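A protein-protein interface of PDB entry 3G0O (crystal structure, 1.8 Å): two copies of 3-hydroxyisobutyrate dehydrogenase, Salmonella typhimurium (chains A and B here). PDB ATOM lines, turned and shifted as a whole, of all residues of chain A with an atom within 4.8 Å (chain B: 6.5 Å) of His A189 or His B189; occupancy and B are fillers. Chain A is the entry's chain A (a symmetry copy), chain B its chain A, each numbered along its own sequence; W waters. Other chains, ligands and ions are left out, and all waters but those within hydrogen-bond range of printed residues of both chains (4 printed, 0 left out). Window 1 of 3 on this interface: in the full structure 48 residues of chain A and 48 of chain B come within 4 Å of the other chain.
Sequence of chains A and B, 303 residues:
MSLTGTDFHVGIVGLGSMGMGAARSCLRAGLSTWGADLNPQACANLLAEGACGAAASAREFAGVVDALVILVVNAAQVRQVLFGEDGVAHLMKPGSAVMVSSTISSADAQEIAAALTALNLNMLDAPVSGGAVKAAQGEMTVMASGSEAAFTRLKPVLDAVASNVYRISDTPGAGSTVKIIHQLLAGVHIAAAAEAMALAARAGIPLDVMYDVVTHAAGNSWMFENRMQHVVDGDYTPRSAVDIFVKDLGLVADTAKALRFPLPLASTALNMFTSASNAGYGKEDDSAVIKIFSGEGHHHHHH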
ATOM      1  N   LEU A 184      32.130 -20.037  10.314  1.00  0.00           N
ATOM      2  CA  LEU A 184      33.238 -20.349   9.420  1.00  0.00           C
ATOM      3  C   LEU A 184      32.616 -20.452   8.025  1.00  0.00           C
ATOM      4  O   LEU A 184      33.110 -19.862   7.062  1.00  0.00           O
ATOM      5  CB  LEU A 184      33.892 -21.685   9.812  1.00  0.00           C
ATOM      6  CG  LEU A 184      35.092 -22.191   8.987  1.00  0.00           C
ATOM      7  CD1 LEU A 184      35.783 -23.320   9.744  1.00  0.00           C
ATOM      8  CD2 LEU A 184      34.649 -22.675   7.611  1.00  0.00           C
ATOM      9  N   LEU A 185      31.515 -21.190   7.930  1.00  0.00           N
ATOM     10  CA  LEU A 185      30.828 -21.359   6.652  1.00  0.00           C
ATOM     11  C   LEU A 185      30.237 -20.040   6.145  1.00  0.00           C
ATOM     12  O   LEU A 185      30.399 -19.689   4.980  1.00  0.00           O
ATOM     13  CB  LEU A 185      29.727 -22.416   6.782  1.00  0.00           C
ATOM     14  CG  LEU A 185      30.223 -23.865   6.887  1.00  0.00           C
ATOM     15  CD1 LEU A 185      29.075 -24.790   7.255  1.00  0.00           C
ATOM     16  CD2 LEU A 185      30.846 -24.280   5.559  1.00  0.00           C
ATOM     17  N   ALA A 186      29.552 -19.311   7.020  1.00  0.00           N
ATOM     18  CA  ALA A 186      28.951 -18.041   6.625  1.00  0.00           C
ATOM     19  C   ALA A 186      30.029 -17.103   6.079  1.00  0.00           C
ATOM     20  O   ALA A 186      29.864 -16.509   5.017  1.00  0.00           O
ATOM     21  CB  ALA A 186      28.247 -17.392   7.823  1.00  0.00           C
ATOM     22  N   GLY A 187      31.137 -16.991   6.810  1.00  0.00           N
ATOM     23  CA  GLY A 187      32.218 -16.113   6.394  1.00  0.00           C
ATOM     24  C   GLY A 187      32.889 -16.521   5.097  1.00  0.00           C
ATOM     25  O   GLY A 187      33.119 -15.682   4.221  1.00  0.00           O
ATOM     26  N   VAL A 188      33.220 -17.803   4.978  1.00  0.00           N
ATOM     27  CA  VAL A 188      33.864 -18.294   3.769  1.00  0.00           C
ATOM     28  C   VAL A 188      32.927 -18.147   2.576  1.00  0.00           C
ATOM     29  O   VAL A 188      33.359 -17.794   1.482  1.00  0.00           O
ATOM     30  CB  VAL A 188      34.276 -19.774   3.916  1.00  0.00           C
ATOM     31  CG1 VAL A 188      34.699 -20.341   2.564  1.00  0.00           C
ATOM     32  CG2 VAL A 188      35.422 -19.892   4.917  1.00  0.00           C
ATOM     33  N   HIS A 189      31.640 -18.405   2.785  1.00  0.00           N
ATOM     34  CA  HIS A 189      30.691 -18.289   1.683  1.00  0.00           C
ATOM     35  C   HIS A 189      30.560 -16.853   1.177  1.00  0.00           C
ATOM     36  O   HIS A 189      30.492 -16.629  -0.032  1.00  0.00           O
ATOM     37  CB  HIS A 189      29.330 -18.859   2.090  1.00  0.00           C
ATOM     38  CG  HIS A 189      29.328 -20.351   2.239  1.00  0.00           C
ATOM     39  ND1 HIS A 189      28.313 -21.038   2.868  1.00  0.00           N
ATOM     40  CD2 HIS A 189      30.239 -21.284   1.870  1.00  0.00           C
ATOM     41  CE1 HIS A 189      28.599 -22.328   2.886  1.00  0.00           C
ATOM     42  NE2 HIS A 189      29.764 -22.503   2.287  1.00  0.00           N
ATOM     43  N   ILE A 190      30.537 -15.874   2.073  1.00  0.00           N
ATOM     44  CA  ILE A 190      30.445 -14.494   1.606  1.00  0.00           C
ATOM     45  C   ILE A 190      31.693 -14.163   0.785  1.00  0.00           C
ATOM     46  O   ILE A 190      31.597 -13.602  -0.307  1.00  0.00           O
ATOM     47  CB  ILE A 190      30.335 -13.483   2.767  1.00  0.00           C
ATOM     48  CG1 ILE A 190      28.994 -13.666   3.490  1.00  0.00           C
ATOM     49  CG2 ILE A 190      30.438 -12.058   2.216  1.00  0.00           C
ATOM     50  CD1 ILE A 190      28.855 -12.843   4.761  1.00  0.00           C
ATOM     51  N   ALA A 191      32.863 -14.524   1.304  1.00  0.00           N
ATOM     52  CA  ALA A 191      34.110 -14.242   0.602  1.00  0.00           C
ATOM     53  C   ALA A 191      34.203 -14.974  -0.737  1.00  0.00           C
ATOM     54  O   ALA A 191      34.672 -14.407  -1.725  1.00  0.00           O
ATOM     55  CB  ALA A 191      35.316 -14.599   1.494  1.00  0.00           C
ATOM     56  N   ALA A 192      33.761 -16.229  -0.775  1.00  0.00           N
ATOM     57  CA  ALA A 192      33.803 -17.002  -2.010  1.00  0.00           C
ATOM     58  C   ALA A 192      32.856 -16.382  -3.035  1.00  0.00           C
ATOM     59  O   ALA A 192      33.183 -16.296  -4.214  1.00  0.00           O
ATOM     60  CB  ALA A 192      33.419 -18.461  -1.739  1.00  0.00           C
ATOM     61  N   ALA A 193      31.687 -15.940  -2.579  1.00  0.00           N
ATOM     62  CA  ALA A 193      30.725 -15.315  -3.483  1.00  0.00           C
ATOM     63  C   ALA A 193      31.373 -14.078  -4.100  1.00  0.00           C
ATOM     64  O   ALA A 193      31.317 -13.871  -5.316  1.00  0.00           O
ATOM     65  CB  ALA A 193      29.456 -14.923  -2.720  1.00  0.00           C
ATOM     66  N   GLY A 219      26.032 -24.302  -7.374  1.00  0.00           N
ATOM     67  CA  GLY A 219      27.039 -23.522  -6.672  1.00  0.00           C
ATOM     68  C   GLY A 219      26.473 -22.450  -5.755  1.00  0.00           C
ATOM     69  O   GLY A 219      27.212 -21.666  -5.160  1.00  0.00           O
ATOM     70  N   ASN A 220      25.154 -22.421  -5.628  1.00  0.00           N
ATOM     71  CA  ASN A 220      24.490 -21.426  -4.797  1.00  0.00           C
ATOM     72  C   ASN A 220      24.719 -21.652  -3.305  1.00  0.00           C
ATOM     73  O   ASN A 220      25.019 -22.764  -2.867  1.00  0.00           O
ATOM     74  CB  ASN A 220      22.986 -21.443  -5.098  1.00  0.00           C
ATOM     75  CG  ASN A 220      22.248 -20.247  -4.516  1.00  0.00           C
ATOM     76  OD1 ASN A 220      22.802 -19.152  -4.391  1.00  0.00           O
ATOM     77  ND2 ASN A 220      20.976 -20.447  -4.180  1.00  0.00           N
ATOM     78  N   SER A 221      24.606 -20.575  -2.536  1.00  0.00           N
ATOM     79  CA  SER A 221      24.727 -20.655  -1.087  1.00  0.00           C
ATOM     80  C   SER A 221      23.763 -19.614  -0.548  1.00  0.00           C
ATOM     81  O   SER A 221      23.398 -18.670  -1.261  1.00  0.00           O
ATOM     82  CB  SER A 221      26.149 -20.345  -0.615  1.00  0.00           C
ATOM     83  OG  SER A 221      26.420 -18.954  -0.650  1.00  0.00           O
ATOM     84  N   MET A 223      24.376 -17.410   1.648  1.00  0.00           N
ATOM     85  CA  MET A 223      25.092 -16.139   1.670  1.00  0.00           C
ATOM     86  C   MET A 223      25.289 -15.533   0.287  1.00  0.00           C
ATOM     87  O   MET A 223      25.248 -14.315   0.135  1.00  0.00           O
ATOM     88  CB  MET A 223      26.441 -16.293   2.383  1.00  0.00           C
ATOM     89  CG  MET A 223      26.293 -16.370   3.893  1.00  0.00           C
ATOM     90  SD  MET A 223      25.416 -14.771   4.613  1.00  0.00           S
ATOM     91  CE  MET A 223      25.850 -15.027   6.485  1.00  0.00           C
ATOM     92  N   LEU B 184      33.866 -22.531  -9.683  1.00  0.00           N
ATOM     93  CA  LEU B 184      34.719 -21.952  -8.652  1.00  0.00           C
ATOM     94  C   LEU B 184      33.907 -22.045  -7.357  1.00  0.00           C
ATOM     95  O   LEU B 184      34.404 -22.499  -6.325  1.00  0.00           O
ATOM     96  CB  LEU B 184      35.040 -20.483  -8.976  1.00  0.00           C
ATOM     97  CG  LEU B 184      35.938 -19.692  -8.005  1.00  0.00           C
ATOM     98  CD1 LEU B 184      36.400 -18.406  -8.681  1.00  0.00           C
ATOM     99  CD2 LEU B 184      35.198 -19.369  -6.711  1.00  0.00           C
ATOM    100  N   LEU B 185      32.647 -21.629  -7.427  1.00  0.00           N
ATOM    101  CA  LEU B 185      31.772 -21.673  -6.258  1.00  0.00           C
ATOM    102  C   LEU B 185      31.490 -23.110  -5.812  1.00  0.00           C
ATOM    103  O   LEU B 185      31.579 -23.427  -4.629  1.00  0.00           O
ATOM    104  CB  LEU B 185      30.458 -20.945  -6.557  1.00  0.00           C
ATOM    105  CG  LEU B 185      30.560 -19.414  -6.620  1.00  0.00           C
ATOM    106  CD1 LEU B 185      29.268 -18.821  -7.158  1.00  0.00           C
ATOM    107  CD2 LEU B 185      30.862 -18.873  -5.228  1.00  0.00           C
ATOM    108  N   ALA B 186      31.150 -23.979  -6.758  1.00  0.00           N
ATOM    109  CA  ALA B 186      30.861 -25.370  -6.426  1.00  0.00           C
ATOM    110  C   ALA B 186      32.064 -25.997  -5.720  1.00  0.00           C
ATOM    111  O   ALA B 186      31.921 -26.634  -4.680  1.00  0.00           O
ATOM    112  CB  ALA B 186      30.525 -26.161  -7.696  1.00  0.00           C
ATOM    113  N   GLY B 187      33.252 -25.797  -6.291  1.00  0.00           N
ATOM    114  CA  GLY B 187      34.460 -26.363  -5.715  1.00  0.00           C
ATOM    115  C   GLY B 187      34.815 -25.815  -4.347  1.00  0.00           C
ATOM    116  O   GLY B 187      35.138 -26.578  -3.432  1.00  0.00           O
ATOM    117  N   VAL B 188      34.773 -24.494  -4.207  1.00  0.00           N
ATOM    118  CA  VAL B 188      35.092 -23.872  -2.931  1.00  0.00           C
ATOM    119  C   VAL B 188      34.074 -24.285  -1.875  1.00  0.00           C
ATOM    120  O   VAL B 188      34.430 -24.530  -0.726  1.00  0.00           O
ATOM    121  CB  VAL B 188      35.111 -22.332  -3.048  1.00  0.00           C
ATOM    122  CG1 VAL B 188      35.179 -21.698  -1.662  1.00  0.00           C
ATOM    123  CG2 VAL B 188      36.309 -21.895  -3.886  1.00  0.00           C
ATOM    124  N   HIS B 189      32.806 -24.374  -2.262  1.00  0.00           N
ATOM    125  CA  HIS B 189      31.780 -24.759  -1.298  1.00  0.00           C
ATOM    126  C   HIS B 189      31.969 -26.188  -0.788  1.00  0.00           C
ATOM    127  O   HIS B 189      31.799 -26.444   0.404  1.00  0.00           O
ATOM    128  CB  HIS B 189      30.385 -24.565  -1.897  1.00  0.00           C
ATOM    129  CG  HIS B 189      30.007 -23.125  -2.073  1.00  0.00           C
ATOM    130  ND1 HIS B 189      28.941 -22.722  -2.848  1.00  0.00           N
ATOM    131  CD2 HIS B 189      30.577 -21.990  -1.601  1.00  0.00           C
ATOM    132  CE1 HIS B 189      28.874 -21.402  -2.850  1.00  0.00           C
ATOM    133  NE2 HIS B 189      29.856 -20.934  -2.101  1.00  0.00           N
ATOM    134  N   ILE B 190      32.330 -27.121  -1.661  1.00  0.00           N
ATOM    135  CA  ILE B 190      32.546 -28.484  -1.185  1.00  0.00           C
ATOM    136  C   ILE B 190      33.713 -28.486  -0.195  1.00  0.00           C
ATOM    137  O   ILE B 190      33.622 -29.072   0.884  1.00  0.00           O
ATOM    138  CB  ILE B 190      32.868 -29.466  -2.331  1.00  0.00           C
ATOM    139  CG1 ILE B 190      31.639 -29.634  -3.234  1.00  0.00           C
ATOM    140  CG2 ILE B 190      33.271 -30.822  -1.745  1.00  0.00           C
ATOM    141  CD1 ILE B 190      31.898 -30.439  -4.496  1.00  0.00           C
ATOM    142  N   ALA B 191      34.804 -27.817  -0.557  1.00  0.00           N
ATOM    143  CA  ALA B 191      35.973 -27.770   0.314  1.00  0.00           C
ATOM    144  C   ALA B 191      35.684 -27.064   1.640  1.00  0.00           C
ATOM    145  O   ALA B 191      36.148 -27.505   2.693  1.00  0.00           O
ATOM    146  CB  ALA B 191      37.151 -27.088  -0.411  1.00  0.00           C
ATOM    147  N   ALA B 192      34.923 -25.974   1.593  1.00  0.00           N
ATOM    148  CA  ALA B 192      34.589 -25.240   2.808  1.00  0.00           C
ATOM    149  C   ALA B 192      33.711 -26.109   3.705  1.00  0.00           C
ATOM    150  O   ALA B 192      33.884 -26.127   4.920  1.00  0.00           O
ATOM    151  CB  ALA B 192      33.871 -23.931   2.461  1.00  0.00           C
ATOM    152  N   ALA B 193      32.775 -26.838   3.103  1.00  0.00           N
ATOM    153  CA  ALA B 193      31.900 -27.712   3.878  1.00  0.00           C
ATOM    154  C   ALA B 193      32.764 -28.744   4.601  1.00  0.00           C
ATOM    155  O   ALA B 193      32.599 -28.981   5.802  1.00  0.00           O
ATOM    156  CB  ALA B 193      30.898 -28.415   2.957  1.00  0.00           C
ATOM    157  N   ALA B 194      33.697 -29.343   3.864  1.00  0.00           N
ATOM    158  CA  ALA B 194      34.584 -30.350   4.429  1.00  0.00           C
ATOM    159  C   ALA B 194      35.413 -29.779   5.568  1.00  0.00           C
ATOM    160  O   ALA B 194      35.574 -30.413   6.610  1.00  0.00           O
ATOM    161  CB  ALA B 194      35.502 -30.908   3.352  1.00  0.00           C
ATOM    162  N   VAL B 214      23.429 -26.511  10.156  1.00  0.00           N
ATOM    163  CA  VAL B 214      23.828 -25.768   8.972  1.00  0.00           C
ATOM    164  C   VAL B 214      22.747 -25.738   7.898  1.00  0.00           C
ATOM    165  O   VAL B 214      22.448 -24.680   7.346  1.00  0.00           O
ATOM    166  CB  VAL B 214      25.123 -26.334   8.348  1.00  0.00           C
ATOM    167  CG1 VAL B 214      25.409 -25.629   7.028  1.00  0.00           C
ATOM    168  CG2 VAL B 214      26.291 -26.146   9.311  1.00  0.00           C
ATOM    169  N   ALA B 218      21.996 -19.795   8.004  1.00  0.00           N
ATOM    170  CA  ALA B 218      22.522 -18.928   6.958  1.00  0.00           C
ATOM    171  C   ALA B 218      23.840 -19.383   6.327  1.00  0.00           C
ATOM    172  O   ALA B 218      24.246 -18.847   5.296  1.00  0.00           O
ATOM    173  CB  ALA B 218      22.668 -17.504   7.500  1.00  0.00           C
ATOM    174  N   GLY B 219      24.498 -20.373   6.925  1.00  0.00           N
ATOM    175  CA  GLY B 219      25.763 -20.844   6.381  1.00  0.00           C
ATOM    176  C   GLY B 219      25.633 -22.011   5.416  1.00  0.00           C
ATOM    177  O   GLY B 219      26.628 -22.559   4.942  1.00  0.00           O
ATOM    178  N   ASN B 220      24.400 -22.388   5.111  1.00  0.00           N
ATOM    179  CA  ASN B 220      24.144 -23.508   4.216  1.00  0.00           C
ATOM    180  C   ASN B 220      24.506 -23.202   2.766  1.00  0.00           C
ATOM    181  O   ASN B 220      24.556 -22.042   2.352  1.00  0.00           O
ATOM    182  CB  ASN B 220      22.663 -23.897   4.309  1.00  0.00           C
ATOM    183  CG  ASN B 220      22.357 -25.236   3.653  1.00  0.00           C
ATOM    184  OD1 ASN B 220      23.195 -26.141   3.626  1.00  0.00           O
ATOM    185  ND2 ASN B 220      21.136 -25.375   3.144  1.00  0.00           N
ATOM    186  N   SER B 221      24.790 -24.255   2.008  1.00  0.00           N
ATOM    187  CA  SER B 221      25.082 -24.119   0.588  1.00  0.00           C
ATOM    188  C   SER B 221      24.513 -25.368  -0.058  1.00  0.00           C
ATOM    189  O   SER B 221      24.319 -26.389   0.616  1.00  0.00           O
ATOM    190  CB  SER B 221      26.586 -24.030   0.320  1.00  0.00           C
ATOM    191  OG  SER B 221      27.210 -25.299   0.418  1.00  0.00           O
ATOM    192  N   TRP B 222      24.233 -25.294  -1.352  1.00  0.00           N
ATOM    193  CA  TRP B 222      23.695 -26.452  -2.049  1.00  0.00           C
ATOM    194  C   TRP B 222      24.700 -27.597  -1.929  1.00  0.00           C
ATOM    195  O   TRP B 222      24.325 -28.738  -1.670  1.00  0.00           O
ATOM    196  CB  TRP B 222      23.452 -26.134  -3.527  1.00  0.00           C
ATOM    197  CG  TRP B 222      22.602 -27.165  -4.212  1.00  0.00           C
ATOM    198  CD1 TRP B 222      21.245 -27.134  -4.375  1.00  0.00           C
ATOM    199  CD2 TRP B 222      23.046 -28.410  -4.776  1.00  0.00           C
ATOM    200  NE1 TRP B 222      20.817 -28.283  -5.004  1.00  0.00           N
ATOM    201  CE2 TRP B 222      21.898 -29.079  -5.260  1.00  0.00           C
ATOM    202  CE3 TRP B 222      24.298 -29.021  -4.918  1.00  0.00           C
ATOM    203  CZ2 TRP B 222      21.970 -30.336  -5.875  1.00  0.00           C
ATOM    204  CZ3 TRP B 222      24.367 -30.269  -5.530  1.00  0.00           C
ATOM    205  CH2 TRP B 222      23.209 -30.911  -6.000  1.00  0.00           C
ATOM    206  N   MET B 223      25.984 -27.288  -2.109  1.00  0.00           N
ATOM    207  CA  MET B 223      27.008 -28.322  -2.009  1.00  0.00           C
ATOM    208  C   MET B 223      27.169 -28.880  -0.601  1.00  0.00           C
ATOM    209  O   MET B 223      27.433 -30.068  -0.433  1.00  0.00           O
ATOM    210  CB  MET B 223      28.352 -27.802  -2.534  1.00  0.00           C
ATOM    211  CG  MET B 223      28.397 -27.739  -4.051  1.00  0.00           C
ATOM    212  SD  MET B 223      28.084 -29.500  -4.854  1.00  0.00           S
ATOM    213  CE  MET B 223      28.685 -29.103  -6.654  1.00  0.00           C
ATOM    214  N   PHE B 224      27.023 -28.037   0.416  1.00  0.00           N
ATOM    215  CA  PHE B 224      27.131 -28.530   1.781  1.00  0.00           C
ATOM    216  C   PHE B 224      26.012 -29.546   2.003  1.00  0.00           C
ATOM    217  O   PHE B 224      26.251 -30.680   2.425  1.00  0.00           O
ATOM    218  CB  PHE B 224      26.966 -27.399   2.806  1.00  0.00           C
ATOM    219  CG  PHE B 224      27.041 -27.869   4.236  1.00  0.00           C
ATOM    220  CD1 PHE B 224      28.232 -27.778   4.955  1.00  0.00           C
ATOM    221  CD2 PHE B 224      25.940 -28.473   4.840  1.00  0.00           C
ATOM    222  CE1 PHE B 224      28.329 -28.286   6.254  1.00  0.00           C
ATOM    223  CE2 PHE B 224      26.025 -28.985   6.136  1.00  0.00           C
ATOM    224  CZ  PHE B 224      27.223 -28.893   6.845  1.00  0.00           C
ATOM    225  N   MET B 228      27.758 -33.114   2.207  1.00  0.00           N
ATOM    226  CA  MET B 228      27.987 -33.491   3.596  1.00  0.00           C
ATOM    227  C   MET B 228      27.100 -34.624   4.111  1.00  0.00           C
ATOM    228  O   MET B 228      27.337 -35.159   5.193  1.00  0.00           O
ATOM    229  CB  MET B 228      27.909 -32.267   4.510  1.00  0.00           C
ATOM    230  CG  MET B 228      29.055 -31.270   4.295  1.00  0.00           C
ATOM    231  SD  MET B 228      30.865 -32.024   4.399  1.00  0.00           S
ATOM    232  CE  MET B 228      31.150 -32.417   2.510  1.00  0.00           C
ATOM    233  N   LEU B 265      40.674 -17.874  -2.441  1.00  0.00           N
ATOM    234  CA  LEU B 265      39.925 -19.066  -2.061  1.00  0.00           C
ATOM    235  C   LEU B 265      39.937 -20.208  -3.083  1.00  0.00           C
ATOM    236  O   LEU B 265      40.048 -21.375  -2.708  1.00  0.00           O
ATOM    237  CB  LEU B 265      38.480 -18.685  -1.731  1.00  0.00           C
ATOM    238  CG  LEU B 265      38.309 -17.747  -0.530  1.00  0.00           C
ATOM    239  CD1 LEU B 265      36.870 -17.243  -0.481  1.00  0.00           C
ATOM    240  CD2 LEU B 265      38.672 -18.471   0.766  1.00  0.00           C
ATOM    241  N   ALA B 269      41.268 -24.054  -2.578  1.00  0.00           N
ATOM    242  CA  ALA B 269      40.442 -25.234  -2.823  1.00  0.00           C
ATOM    243  C   ALA B 269      41.130 -26.174  -3.814  1.00  0.00           C
ATOM    244  O   ALA B 269      41.099 -27.393  -3.645  1.00  0.00           O
ATOM    245  CB  ALA B 269      39.073 -24.812  -3.354  1.00  0.00           C
HETATM  246  O   HOH W   1      26.769 -24.838  -3.442  1.00  0.00           O
HETATM  247  O   HOH W   2      28.852 -18.509  -1.611  1.00  0.00           O
HETATM  248  O   HOH W   3      29.518 -25.099   1.710  1.00  0.00           O
HETATM  249  O   HOH W   4      25.596 -19.587   3.121  1.00  0.00           O
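A ring nitrogen (ND1) of His B189 lies close to the backbone carbonyl oxygen of Gly A219, 3.1 Å away. ND1 of His A189 lies close to O of Gly B219 (3.1 Å). The backbone carbonyl oxygen (O) of Asn A220 lies within hydrogen-bond range of the backbone NH (N) of Trp B222.
The backbone carbonyl oxygen of Leu B185 lies close to a ring nitrogen (ND1) of His B189 (3.3 Å). The side-chain hydroxyl (OG) of Ser B221 lies close to the backbone NH (N) of Met B223 (3.4 Å). OG of Ser B221 sits at hydrogen-bond distance from N of Phe B224 (2.7 Å). O of Leu A185 lies close to ND1 of His A189, at 3.3 Å. OG of Ser A221 sits close to N of Met A223.
CA of Ala B193 touches CD2 of Leu A185 (3.96 Å). CG2 of Val B214 touches CD1 of Leu A185, at 3.7 Å. His B189 touches His A189 (CD2 to CD2, 3.6 Å). Asn B220 touches His A189 (O to ND1, 3.9 Å). Ala A191 touches Leu B265 (C to CD1, 3.5 Å). Ala A192 touches Leu B185. Gly A219 touches Leu B185 (O to CB, 3.6 Å). Asn A220 touches His B189. Asn A220 touches Ser B221 (O to CA, 3.7 Å). Met A223 touches Ala B218 (CG to O, 3.5 Å).
His A189 touches just these residues of chain B: His B189 (3.6 Å), Gly B219 (2.9 Å), Asn B220 (3.9 Å) and Ser B221 (3.7 Å). Of the printed residues of chain B, Ala A193 touches Leu B185. Printed residues of chain A within 4 Å of Val B188: Ala A192. Of the printed residues of chain A, Ala B193 touches Leu A185. Printed residues of chain A within 4 Å of Ala B218: Met A223 (3.5 Å). Printed residues of chain A within 4 Å of Leu B265: Ala A191 (3.5 Å) and Ala A192 (3.3 Å). The nearest residue of chain B that does not touch His A189 is Ala B192 (4.4 Å).
Of the 14 printed residues of chain A, 10 touch a printed residue of chain B. Of the 22 printed residues of chain B, 13 touch a printed residue of chain A. Hydrophobic or aromatic side chains of chain B within 4 Å of the printed part of chain A: Leu B185, Val B188, His B189, Ala B192, Val B214, Trp B222, Phe B224 and Leu B265. Along chain B the printed residues that touch a printed residue of chain A span positions 185 to 265.
Leu A185 touches Ala B192, and with the chains exchanged Ala A192 touches Leu B185. Leu A185 touches Gly B219, and with the chains exchanged Gly A219 touches Leu B185. His A189 touches Ser B221, and with the chains exchanged Ser A221 touches His B189. Ser A221 touches its own counterpart, Ser B221. Of the 24 pairs that touch across the chains among the printed residues, 18 have their exchanged pair printed and touching as well.
Water W2 lies within hydrogen-bond range of the side-chain hydroxyl of Ser A221 (2.7 Å), a ring nitrogen (NE2) of His B189 (2.7 Å) and the backbone carbonyl oxygen of His A189 (3.0 Å). Water W3 lies within hydrogen-bond range of OG of Ser B221 (2.7 Å), NE2 of His A189 (2.7 Å) and O of His B189 (3.0 Å). Water W4 lies within hydrogen-bond range of the backbone carbonyl oxygen of Ala B218, the backbone carbonyl oxygen of Asn B220, the backbone NH of Met A223 and a ring nitrogen (ND1) of His A189. Water W1 lies within hydrogen-bond range of the backbone carbonyl oxygen of Asn A220, the backbone NH of Met B223, a ring nitrogen (ND1) of His B189 and the backbone NH of Trp B222.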
